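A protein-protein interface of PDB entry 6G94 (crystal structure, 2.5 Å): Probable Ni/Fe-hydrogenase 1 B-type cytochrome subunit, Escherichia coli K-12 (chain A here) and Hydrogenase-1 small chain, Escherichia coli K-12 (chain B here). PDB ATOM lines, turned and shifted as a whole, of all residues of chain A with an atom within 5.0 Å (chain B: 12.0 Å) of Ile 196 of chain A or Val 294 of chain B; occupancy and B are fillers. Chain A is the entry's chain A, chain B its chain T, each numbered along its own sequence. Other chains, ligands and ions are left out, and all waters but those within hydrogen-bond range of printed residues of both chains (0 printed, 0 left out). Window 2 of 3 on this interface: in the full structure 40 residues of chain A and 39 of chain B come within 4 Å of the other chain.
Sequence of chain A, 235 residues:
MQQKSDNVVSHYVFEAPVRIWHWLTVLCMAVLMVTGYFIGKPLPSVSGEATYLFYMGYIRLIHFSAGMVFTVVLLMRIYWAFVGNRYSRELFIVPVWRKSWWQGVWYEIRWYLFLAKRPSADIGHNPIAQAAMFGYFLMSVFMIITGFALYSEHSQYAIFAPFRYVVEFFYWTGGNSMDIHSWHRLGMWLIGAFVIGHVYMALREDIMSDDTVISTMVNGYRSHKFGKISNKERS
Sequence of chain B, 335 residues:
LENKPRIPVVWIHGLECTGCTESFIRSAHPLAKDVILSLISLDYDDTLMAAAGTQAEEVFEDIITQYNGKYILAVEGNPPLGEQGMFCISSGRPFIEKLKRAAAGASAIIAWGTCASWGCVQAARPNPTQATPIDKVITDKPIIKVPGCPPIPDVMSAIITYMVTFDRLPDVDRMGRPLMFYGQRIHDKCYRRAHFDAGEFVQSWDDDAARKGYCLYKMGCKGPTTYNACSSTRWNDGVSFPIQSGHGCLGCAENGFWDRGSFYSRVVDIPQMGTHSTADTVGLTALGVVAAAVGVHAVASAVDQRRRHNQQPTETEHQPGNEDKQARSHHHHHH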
ATOM      1  N   GLY A 192     -11.250  -0.319  16.369  1.00  0.00           N
ATOM      2  CA  GLY A 192     -11.084  -1.374  17.368  1.00  0.00           C
ATOM      3  C   GLY A 192     -11.722  -1.041  18.709  1.00  0.00           C
ATOM      4  O   GLY A 192     -12.124  -1.944  19.461  1.00  0.00           O
ATOM      5  N   ALA A 193     -11.822   0.257  19.010  1.00  0.00           N
ATOM      6  CA  ALA A 193     -12.521   0.740  20.206  1.00  0.00           C
ATOM      7  C   ALA A 193     -14.006   0.422  20.126  1.00  0.00           C
ATOM      8  O   ALA A 193     -14.507  -0.282  20.997  1.00  0.00           O
ATOM      9  CB  ALA A 193     -12.296   2.230  20.426  1.00  0.00           C
ATOM     10  N   PHE A 194     -14.696   0.919  19.086  1.00  0.00           N
ATOM     11  CA  PHE A 194     -16.120   0.567  18.823  1.00  0.00           C
ATOM     12  C   PHE A 194     -16.353  -0.923  18.905  1.00  0.00           C
ATOM     13  O   PHE A 194     -17.210  -1.370  19.640  1.00  0.00           O
ATOM     14  CB  PHE A 194     -16.626   1.051  17.456  1.00  0.00           C
ATOM     15  CG  PHE A 194     -16.476   2.536  17.235  1.00  0.00           C
ATOM     16  CD1 PHE A 194     -16.519   3.436  18.307  1.00  0.00           C
ATOM     17  CD2 PHE A 194     -16.281   3.049  15.944  1.00  0.00           C
ATOM     18  CE1 PHE A 194     -16.370   4.810  18.098  1.00  0.00           C
ATOM     19  CE2 PHE A 194     -16.132   4.426  15.732  1.00  0.00           C
ATOM     20  CZ  PHE A 194     -16.182   5.305  16.811  1.00  0.00           C
ATOM     21  N   VAL A 195     -15.593  -1.675  18.122  1.00  0.00           N
ATOM     22  CA  VAL A 195     -15.618  -3.135  18.148  1.00  0.00           C
ATOM     23  C   VAL A 195     -15.547  -3.717  19.572  1.00  0.00           C
ATOM     24  O   VAL A 195     -16.288  -4.646  19.866  1.00  0.00           O
ATOM     25  CB  VAL A 195     -14.527  -3.745  17.225  1.00  0.00           C
ATOM     26  CG1 VAL A 195     -14.339  -5.235  17.479  1.00  0.00           C
ATOM     27  CG2 VAL A 195     -14.889  -3.508  15.763  1.00  0.00           C
ATOM     28  N   ILE A 196     -14.713  -3.180  20.465  1.00  0.00           N
ATOM     29  CA  ILE A 196     -14.721  -3.687  21.857  1.00  0.00           C
ATOM     30  C   ILE A 196     -16.047  -3.359  22.555  1.00  0.00           C
ATOM     31  O   ILE A 196     -16.583  -4.176  23.305  1.00  0.00           O
ATOM     32  CB  ILE A 196     -13.530  -3.169  22.693  1.00  0.00           C
ATOM     33  CG1 ILE A 196     -12.234  -3.832  22.227  1.00  0.00           C
ATOM     34  CG2 ILE A 196     -13.734  -3.452  24.172  1.00  0.00           C
ATOM     35  CD1 ILE A 196     -11.009  -3.407  22.999  1.00  0.00           C
ATOM     36  N   GLY A 197     -16.560  -2.161  22.293  1.00  0.00           N
ATOM     37  CA  GLY A 197     -17.879  -1.751  22.738  1.00  0.00           C
ATOM     38  C   GLY A 197     -18.963  -2.571  22.060  1.00  0.00           C
ATOM     39  O   GLY A 197     -19.658  -3.344  22.734  1.00  0.00           O
ATOM     40  N   HIS A 198     -19.073  -2.425  20.736  1.00  0.00           N
ATOM     41  CA  HIS A 198     -20.089  -3.132  19.965  1.00  0.00           C
ATOM     42  C   HIS A 198     -20.099  -4.621  20.270  1.00  0.00           C
ATOM     43  O   HIS A 198     -21.172  -5.174  20.368  1.00  0.00           O
ATOM     44  CB  HIS A 198     -20.014  -2.861  18.446  1.00  0.00           C
ATOM     45  CG  HIS A 198     -21.193  -3.409  17.681  1.00  0.00           C
ATOM     46  ND1 HIS A 198     -22.484  -2.946  17.863  1.00  0.00           N
ATOM     47  CD2 HIS A 198     -21.279  -4.406  16.759  1.00  0.00           C
ATOM     48  CE1 HIS A 198     -23.309  -3.620  17.075  1.00  0.00           C
ATOM     49  NE2 HIS A 198     -22.603  -4.510  16.394  1.00  0.00           N
ATOM     50  N   VAL A 199     -18.953  -5.260  20.463  1.00  0.00           N
ATOM     51  CA  VAL A 199     -18.968  -6.671  20.879  1.00  0.00           C
ATOM     52  C   VAL A 199     -19.500  -6.876  22.303  1.00  0.00           C
ATOM     53  O   VAL A 199     -20.288  -7.787  22.513  1.00  0.00           O
ATOM     54  CB  VAL A 199     -17.622  -7.407  20.659  1.00  0.00           C
ATOM     55  CG1 VAL A 199     -17.594  -8.759  21.357  1.00  0.00           C
ATOM     56  CG2 VAL A 199     -17.385  -7.624  19.176  1.00  0.00           C
ATOM     57  N   TYR A 200     -19.086  -6.053  23.265  1.00  0.00           N
ATOM     58  CA  TYR A 200     -19.601  -6.183  24.632  1.00  0.00           C
ATOM     59  C   TYR A 200     -21.075  -5.819  24.693  1.00  0.00           C
ATOM     60  O   TYR A 200     -21.830  -6.394  25.476  1.00  0.00           O
ATOM     61  CB  TYR A 200     -18.823  -5.325  25.627  1.00  0.00           C
ATOM     62  CG  TYR A 200     -19.560  -5.078  26.941  1.00  0.00           C
ATOM     63  CD1 TYR A 200     -19.583  -6.041  27.935  1.00  0.00           C
ATOM     64  CD2 TYR A 200     -20.252  -3.884  27.169  1.00  0.00           C
ATOM     65  CE1 TYR A 200     -20.258  -5.829  29.119  1.00  0.00           C
ATOM     66  CE2 TYR A 200     -20.928  -3.664  28.352  1.00  0.00           C
ATOM     67  CZ  TYR A 200     -20.932  -4.646  29.319  1.00  0.00           C
ATOM     68  N   MET A 201     -21.469  -4.846  23.883  1.00  0.00           N
ATOM     69  CA  MET A 201     -22.856  -4.415  23.859  1.00  0.00           C
ATOM     70  C   MET A 201     -23.740  -5.504  23.256  1.00  0.00           C
ATOM     71  O   MET A 201     -24.864  -5.710  23.719  1.00  0.00           O
ATOM     72  CB  MET A 201     -23.001  -3.080  23.123  1.00  0.00           C
ATOM     73  CG  MET A 201     -24.439  -2.597  23.004  1.00  0.00           C
ATOM     74  SD  MET A 201     -24.656  -0.815  23.156  1.00  0.00           S
ATOM     75  CE  MET A 201     -26.434  -0.737  23.468  1.00  0.00           C
ATOM     76  N   VAL B 282      -2.358   7.500  21.411  1.00  0.00           N
ATOM     77  CA  VAL B 282      -3.741   7.951  21.369  1.00  0.00           C
ATOM     78  C   VAL B 282      -4.694   6.779  21.086  1.00  0.00           C
ATOM     79  O   VAL B 282      -5.777   6.714  21.635  1.00  0.00           O
ATOM     80  CB  VAL B 282      -3.919   9.075  20.320  1.00  0.00           C
ATOM     81  CG1 VAL B 282      -5.329   9.652  20.364  1.00  0.00           C
ATOM     82  CG2 VAL B 282      -2.926  10.176  20.569  1.00  0.00           C
ATOM     83  N   GLY B 283      -4.267   5.835  20.264  1.00  0.00           N
ATOM     84  CA  GLY B 283      -5.112   4.718  19.902  1.00  0.00           C
ATOM     85  C   GLY B 283      -5.282   3.690  21.000  1.00  0.00           C
ATOM     86  O   GLY B 283      -6.388   3.280  21.318  1.00  0.00           O
ATOM     87  N   LEU B 284      -4.179   3.270  21.590  1.00  0.00           N
ATOM     88  CA  LEU B 284      -4.237   2.299  22.659  1.00  0.00           C
ATOM     89  C   LEU B 284      -4.875   2.871  23.910  1.00  0.00           C
ATOM     90  O   LEU B 284      -5.482   2.131  24.665  1.00  0.00           O
ATOM     91  CB  LEU B 284      -2.837   1.820  22.997  1.00  0.00           C
ATOM     92  CG  LEU B 284      -2.474   0.375  22.688  1.00  0.00           C
ATOM     93  CD1 LEU B 284      -2.947  -0.048  21.309  1.00  0.00           C
ATOM     94  CD2 LEU B 284      -0.971   0.187  22.823  1.00  0.00           C
ATOM     95  N   THR B 285      -4.718   4.174  24.145  1.00  0.00           N
ATOM     96  CA  THR B 285      -5.391   4.857  25.262  1.00  0.00           C
ATOM     97  C   THR B 285      -6.918   4.761  25.126  1.00  0.00           C
ATOM     98  O   THR B 285      -7.626   4.499  26.095  1.00  0.00           O
ATOM     99  CB  THR B 285      -4.979   6.350  25.359  1.00  0.00           C
ATOM    100  OG1 THR B 285      -3.609   6.450  25.778  1.00  0.00           O
ATOM    101  CG2 THR B 285      -5.888   7.122  26.349  1.00  0.00           C
ATOM    102  N   ALA B 286      -7.405   4.963  23.906  1.00  0.00           N
ATOM    103  CA  ALA B 286      -8.827   4.905  23.625  1.00  0.00           C
ATOM    104  C   ALA B 286      -9.336   3.465  23.729  1.00  0.00           C
ATOM    105  O   ALA B 286     -10.463   3.251  24.167  1.00  0.00           O
ATOM    106  CB  ALA B 286      -9.120   5.493  22.253  1.00  0.00           C
ATOM    107  N   LEU B 287      -8.502   2.491  23.343  1.00  0.00           N
ATOM    108  CA  LEU B 287      -8.837   1.054  23.438  1.00  0.00           C
ATOM    109  C   LEU B 287      -8.921   0.574  24.891  1.00  0.00           C
ATOM    110  O   LEU B 287      -9.766  -0.251  25.247  1.00  0.00           O
ATOM    111  CB  LEU B 287      -7.812   0.202  22.669  1.00  0.00           C
ATOM    112  CG  LEU B 287      -8.241  -1.132  22.065  1.00  0.00           C
ATOM    113  CD1 LEU B 287      -9.168  -0.836  20.911  1.00  0.00           C
ATOM    114  CD2 LEU B 287      -7.063  -1.981  21.610  1.00  0.00           C
ATOM    115  N   GLY B 288      -8.040   1.098  25.725  1.00  0.00           N
ATOM    116  CA  GLY B 288      -8.023   0.753  27.123  1.00  0.00           C
ATOM    117  C   GLY B 288      -9.089   1.493  27.897  1.00  0.00           C
ATOM    118  O   GLY B 288      -9.447   1.085  28.999  1.00  0.00           O
ATOM    119  N   VAL B 289      -9.598   2.582  27.330  1.00  0.00           N
ATOM    120  CA  VAL B 289     -10.639   3.384  27.981  1.00  0.00           C
ATOM    121  C   VAL B 289     -12.052   2.804  27.755  1.00  0.00           C
ATOM    122  O   VAL B 289     -12.944   2.936  28.597  1.00  0.00           O
ATOM    123  CB  VAL B 289     -10.441   4.882  27.647  1.00  0.00           C
ATOM    124  CG1 VAL B 289     -11.721   5.630  27.337  1.00  0.00           C
ATOM    125  CG2 VAL B 289      -9.693   5.537  28.771  1.00  0.00           C
ATOM    126  N   VAL B 290     -12.226   2.130  26.624  1.00  0.00           N
ATOM    127  CA  VAL B 290     -13.473   1.439  26.332  1.00  0.00           C
ATOM    128  C   VAL B 290     -13.512   0.131  27.110  1.00  0.00           C
ATOM    129  O   VAL B 290     -14.533  -0.218  27.669  1.00  0.00           O
ATOM    130  CB  VAL B 290     -13.669   1.238  24.822  1.00  0.00           C
ATOM    131  CG1 VAL B 290     -14.808   0.280  24.531  1.00  0.00           C
ATOM    132  CG2 VAL B 290     -13.928   2.577  24.154  1.00  0.00           C
ATOM    133  N   ALA B 291     -12.375  -0.549  27.188  1.00  0.00           N
ATOM    134  CA  ALA B 291     -12.234  -1.774  27.975  1.00  0.00           C
ATOM    135  C   ALA B 291     -12.553  -1.508  29.436  1.00  0.00           C
ATOM    136  O   ALA B 291     -13.076  -2.383  30.125  1.00  0.00           O
ATOM    137  CB  ALA B 291     -10.834  -2.345  27.840  1.00  0.00           C
ATOM    138  N   ALA B 292     -12.248  -0.297  29.894  1.00  0.00           N
ATOM    139  CA  ALA B 292     -12.573   0.134  31.242  1.00  0.00           C
ATOM    140  C   ALA B 292     -14.075   0.268  31.415  1.00  0.00           C
ATOM    141  O   ALA B 292     -14.625  -0.229  32.378  1.00  0.00           O
ATOM    142  CB  ALA B 292     -11.896   1.455  31.547  1.00  0.00           C
ATOM    143  N   ALA B 293     -14.727   0.947  30.477  1.00  0.00           N
ATOM    144  CA  ALA B 293     -16.179   1.111  30.484  1.00  0.00           C
ATOM    145  C   ALA B 293     -16.893  -0.238  30.383  1.00  0.00           C
ATOM    146  O   ALA B 293     -17.837  -0.514  31.118  1.00  0.00           O
ATOM    147  CB  ALA B 293     -16.588   1.999  29.330  1.00  0.00           C
ATOM    148  N   VAL B 294     -16.403  -1.069  29.468  1.00  0.00           N
ATOM    149  CA  VAL B 294     -16.907  -2.409  29.182  1.00  0.00           C
ATOM    150  C   VAL B 294     -16.725  -3.429  30.319  1.00  0.00           C
ATOM    151  O   VAL B 294     -17.390  -4.451  30.348  1.00  0.00           O
ATOM    152  CB  VAL B 294     -16.271  -2.895  27.857  1.00  0.00           C
ATOM    153  CG1 VAL B 294     -16.033  -4.401  27.792  1.00  0.00           C
ATOM    154  CG2 VAL B 294     -17.051  -2.356  26.671  1.00  0.00           C
ATOM    155  N   GLY B 295     -15.848  -3.150  31.272  1.00  0.00           N
ATOM    156  CA  GLY B 295     -15.621  -4.087  32.374  1.00  0.00           C
ATOM    157  C   GLY B 295     -16.097  -3.589  33.722  1.00  0.00           C
ATOM    158  O   GLY B 295     -16.183  -4.361  34.683  1.00  0.00           O
ATOM    159  N   VAL B 296     -16.374  -2.285  33.781  1.00  0.00           N
ATOM    160  CA  VAL B 296     -16.876  -1.616  34.977  1.00  0.00           C
ATOM    161  C   VAL B 296     -18.357  -1.834  34.971  1.00  0.00           C
ATOM    162  O   VAL B 296     -18.934  -2.334  35.934  1.00  0.00           O
ATOM    163  CB  VAL B 296     -16.626  -0.095  34.960  1.00  0.00           C
ATOM    164  N   HIS B 297     -18.966  -1.495  33.844  1.00  0.00           N
ATOM    165  CA  HIS B 297     -20.381  -1.673  33.663  1.00  0.00           C
ATOM    166  C   HIS B 297     -20.777  -3.148  33.825  1.00  0.00           C
ATOM    167  O   HIS B 297     -21.800  -3.437  34.464  1.00  0.00           O
ATOM    168  CB  HIS B 297     -20.786  -1.086  32.326  1.00  0.00           C
ATOM    169  CG  HIS B 297     -22.087  -1.591  31.810  1.00  0.00           C
ATOM    170  ND1 HIS B 297     -23.191  -0.784  31.657  1.00  0.00           N
ATOM    171  CD2 HIS B 297     -22.469  -2.832  31.436  1.00  0.00           C
ATOM    172  CE1 HIS B 297     -24.195  -1.504  31.195  1.00  0.00           C
ATOM    173  NE2 HIS B 297     -23.783  -2.752  31.057  1.00  0.00           N
ATOM    174  N   ALA B 298     -19.954  -4.078  33.314  1.00  0.00           N
ATOM    175  CA  ALA B 298     -20.184  -5.534  33.448  1.00  0.00           C
ATOM    176  C   ALA B 298     -19.974  -6.185  34.857  1.00  0.00           C
ATOM    177  O   ALA B 298     -19.657  -7.374  34.957  1.00  0.00           O
ATOM    178  CB  ALA B 298     -19.388  -6.285  32.388  1.00  0.00           C
ATOM    179  N   VAL B 299     -20.177  -5.417  35.929  1.00  0.00           N
ATOM    180  CA  VAL B 299     -19.993  -5.884  37.297  1.00  0.00           C
ATOM    181  C   VAL B 299     -21.021  -5.210  38.196  1.00  0.00           C
ATOM    182  O   VAL B 299     -22.149  -4.953  37.775  1.00  0.00           O
ATOM    183  CB  VAL B 299     -18.569  -5.601  37.811  1.00  0.00           C
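CD1 of Leu 287 of chain B touches C of Gly 192 of chain A, at 3.4 Å.
Leu 287 of chain B touches Ala 193 of chain A (CD1 to N, 3.4 Å).
CG1 of Val 290 of chain B touches O of Ala 193 of chain A (3.6 Å).
Ile 196 of chain A touches Leu 287 of chain B (CD1 to CG, 3.7 Å).
Val 290 of chain B touches Ile 196 of chain A.
O of Ile 196 of chain A touches CG2 of Val 294 of chain B (3.9 Å).
Val 290 of chain B touches Gly 197 of chain A (CG1 to N, 3.7 Å).
Val 294 of chain B touches Tyr 200 of chain A.
Tyr 200 of chain A touches His 297 of chain B (CZ to CD2, 3.2 Å).
Ala 298 of chain B touches Tyr 200 of chain A.
Ile 196 of chain A touches three residues of chain B.
Ala 193 of chain A touches just these residues of chain B: Leu 287 and Val 290.
Val 195 of chain A touches none of the printed residues of chain B.
Of chain B, only Val 290 (3.7 Å) comes within 4 Å of Gly 197 of chain A.
No residue of chain B comes within 4 Å of Val 199 of chain A.
Tyr 200 of chain A touches just these residues of chain B: Val 294, His 297 and Ala 298.
Of the printed residues of chain A, His 297 of chain B touches Tyr 200 (3.2 Å).
Of the printed residues of chain A, Ala 298 of chain B touches Tyr 200.
Val 299 of chain B touches none of the printed residues of chain A.
The nearest residue of chain B that does not touch Ile 196 of chain A is Ala 291 of chain B (4.4 Å).
Printed residues of chain A that touch a printed residue of chain B: Gly 192, Ala 193, Ile 196, Gly 197 and Tyr 200.
Of the 18 printed residues of chain B, 5 touch a printed residue of chain A.
Hydrophobic or aromatic side chains of chain B that line the printed part of chain A: Leu 287, Val 290, Val 294, His 297 and Ala 298.
Along chain B the printed residues that touch a printed residue of chain A span positions 287 to 298.
Among the printed residues, 10 pairs touch across the chains.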
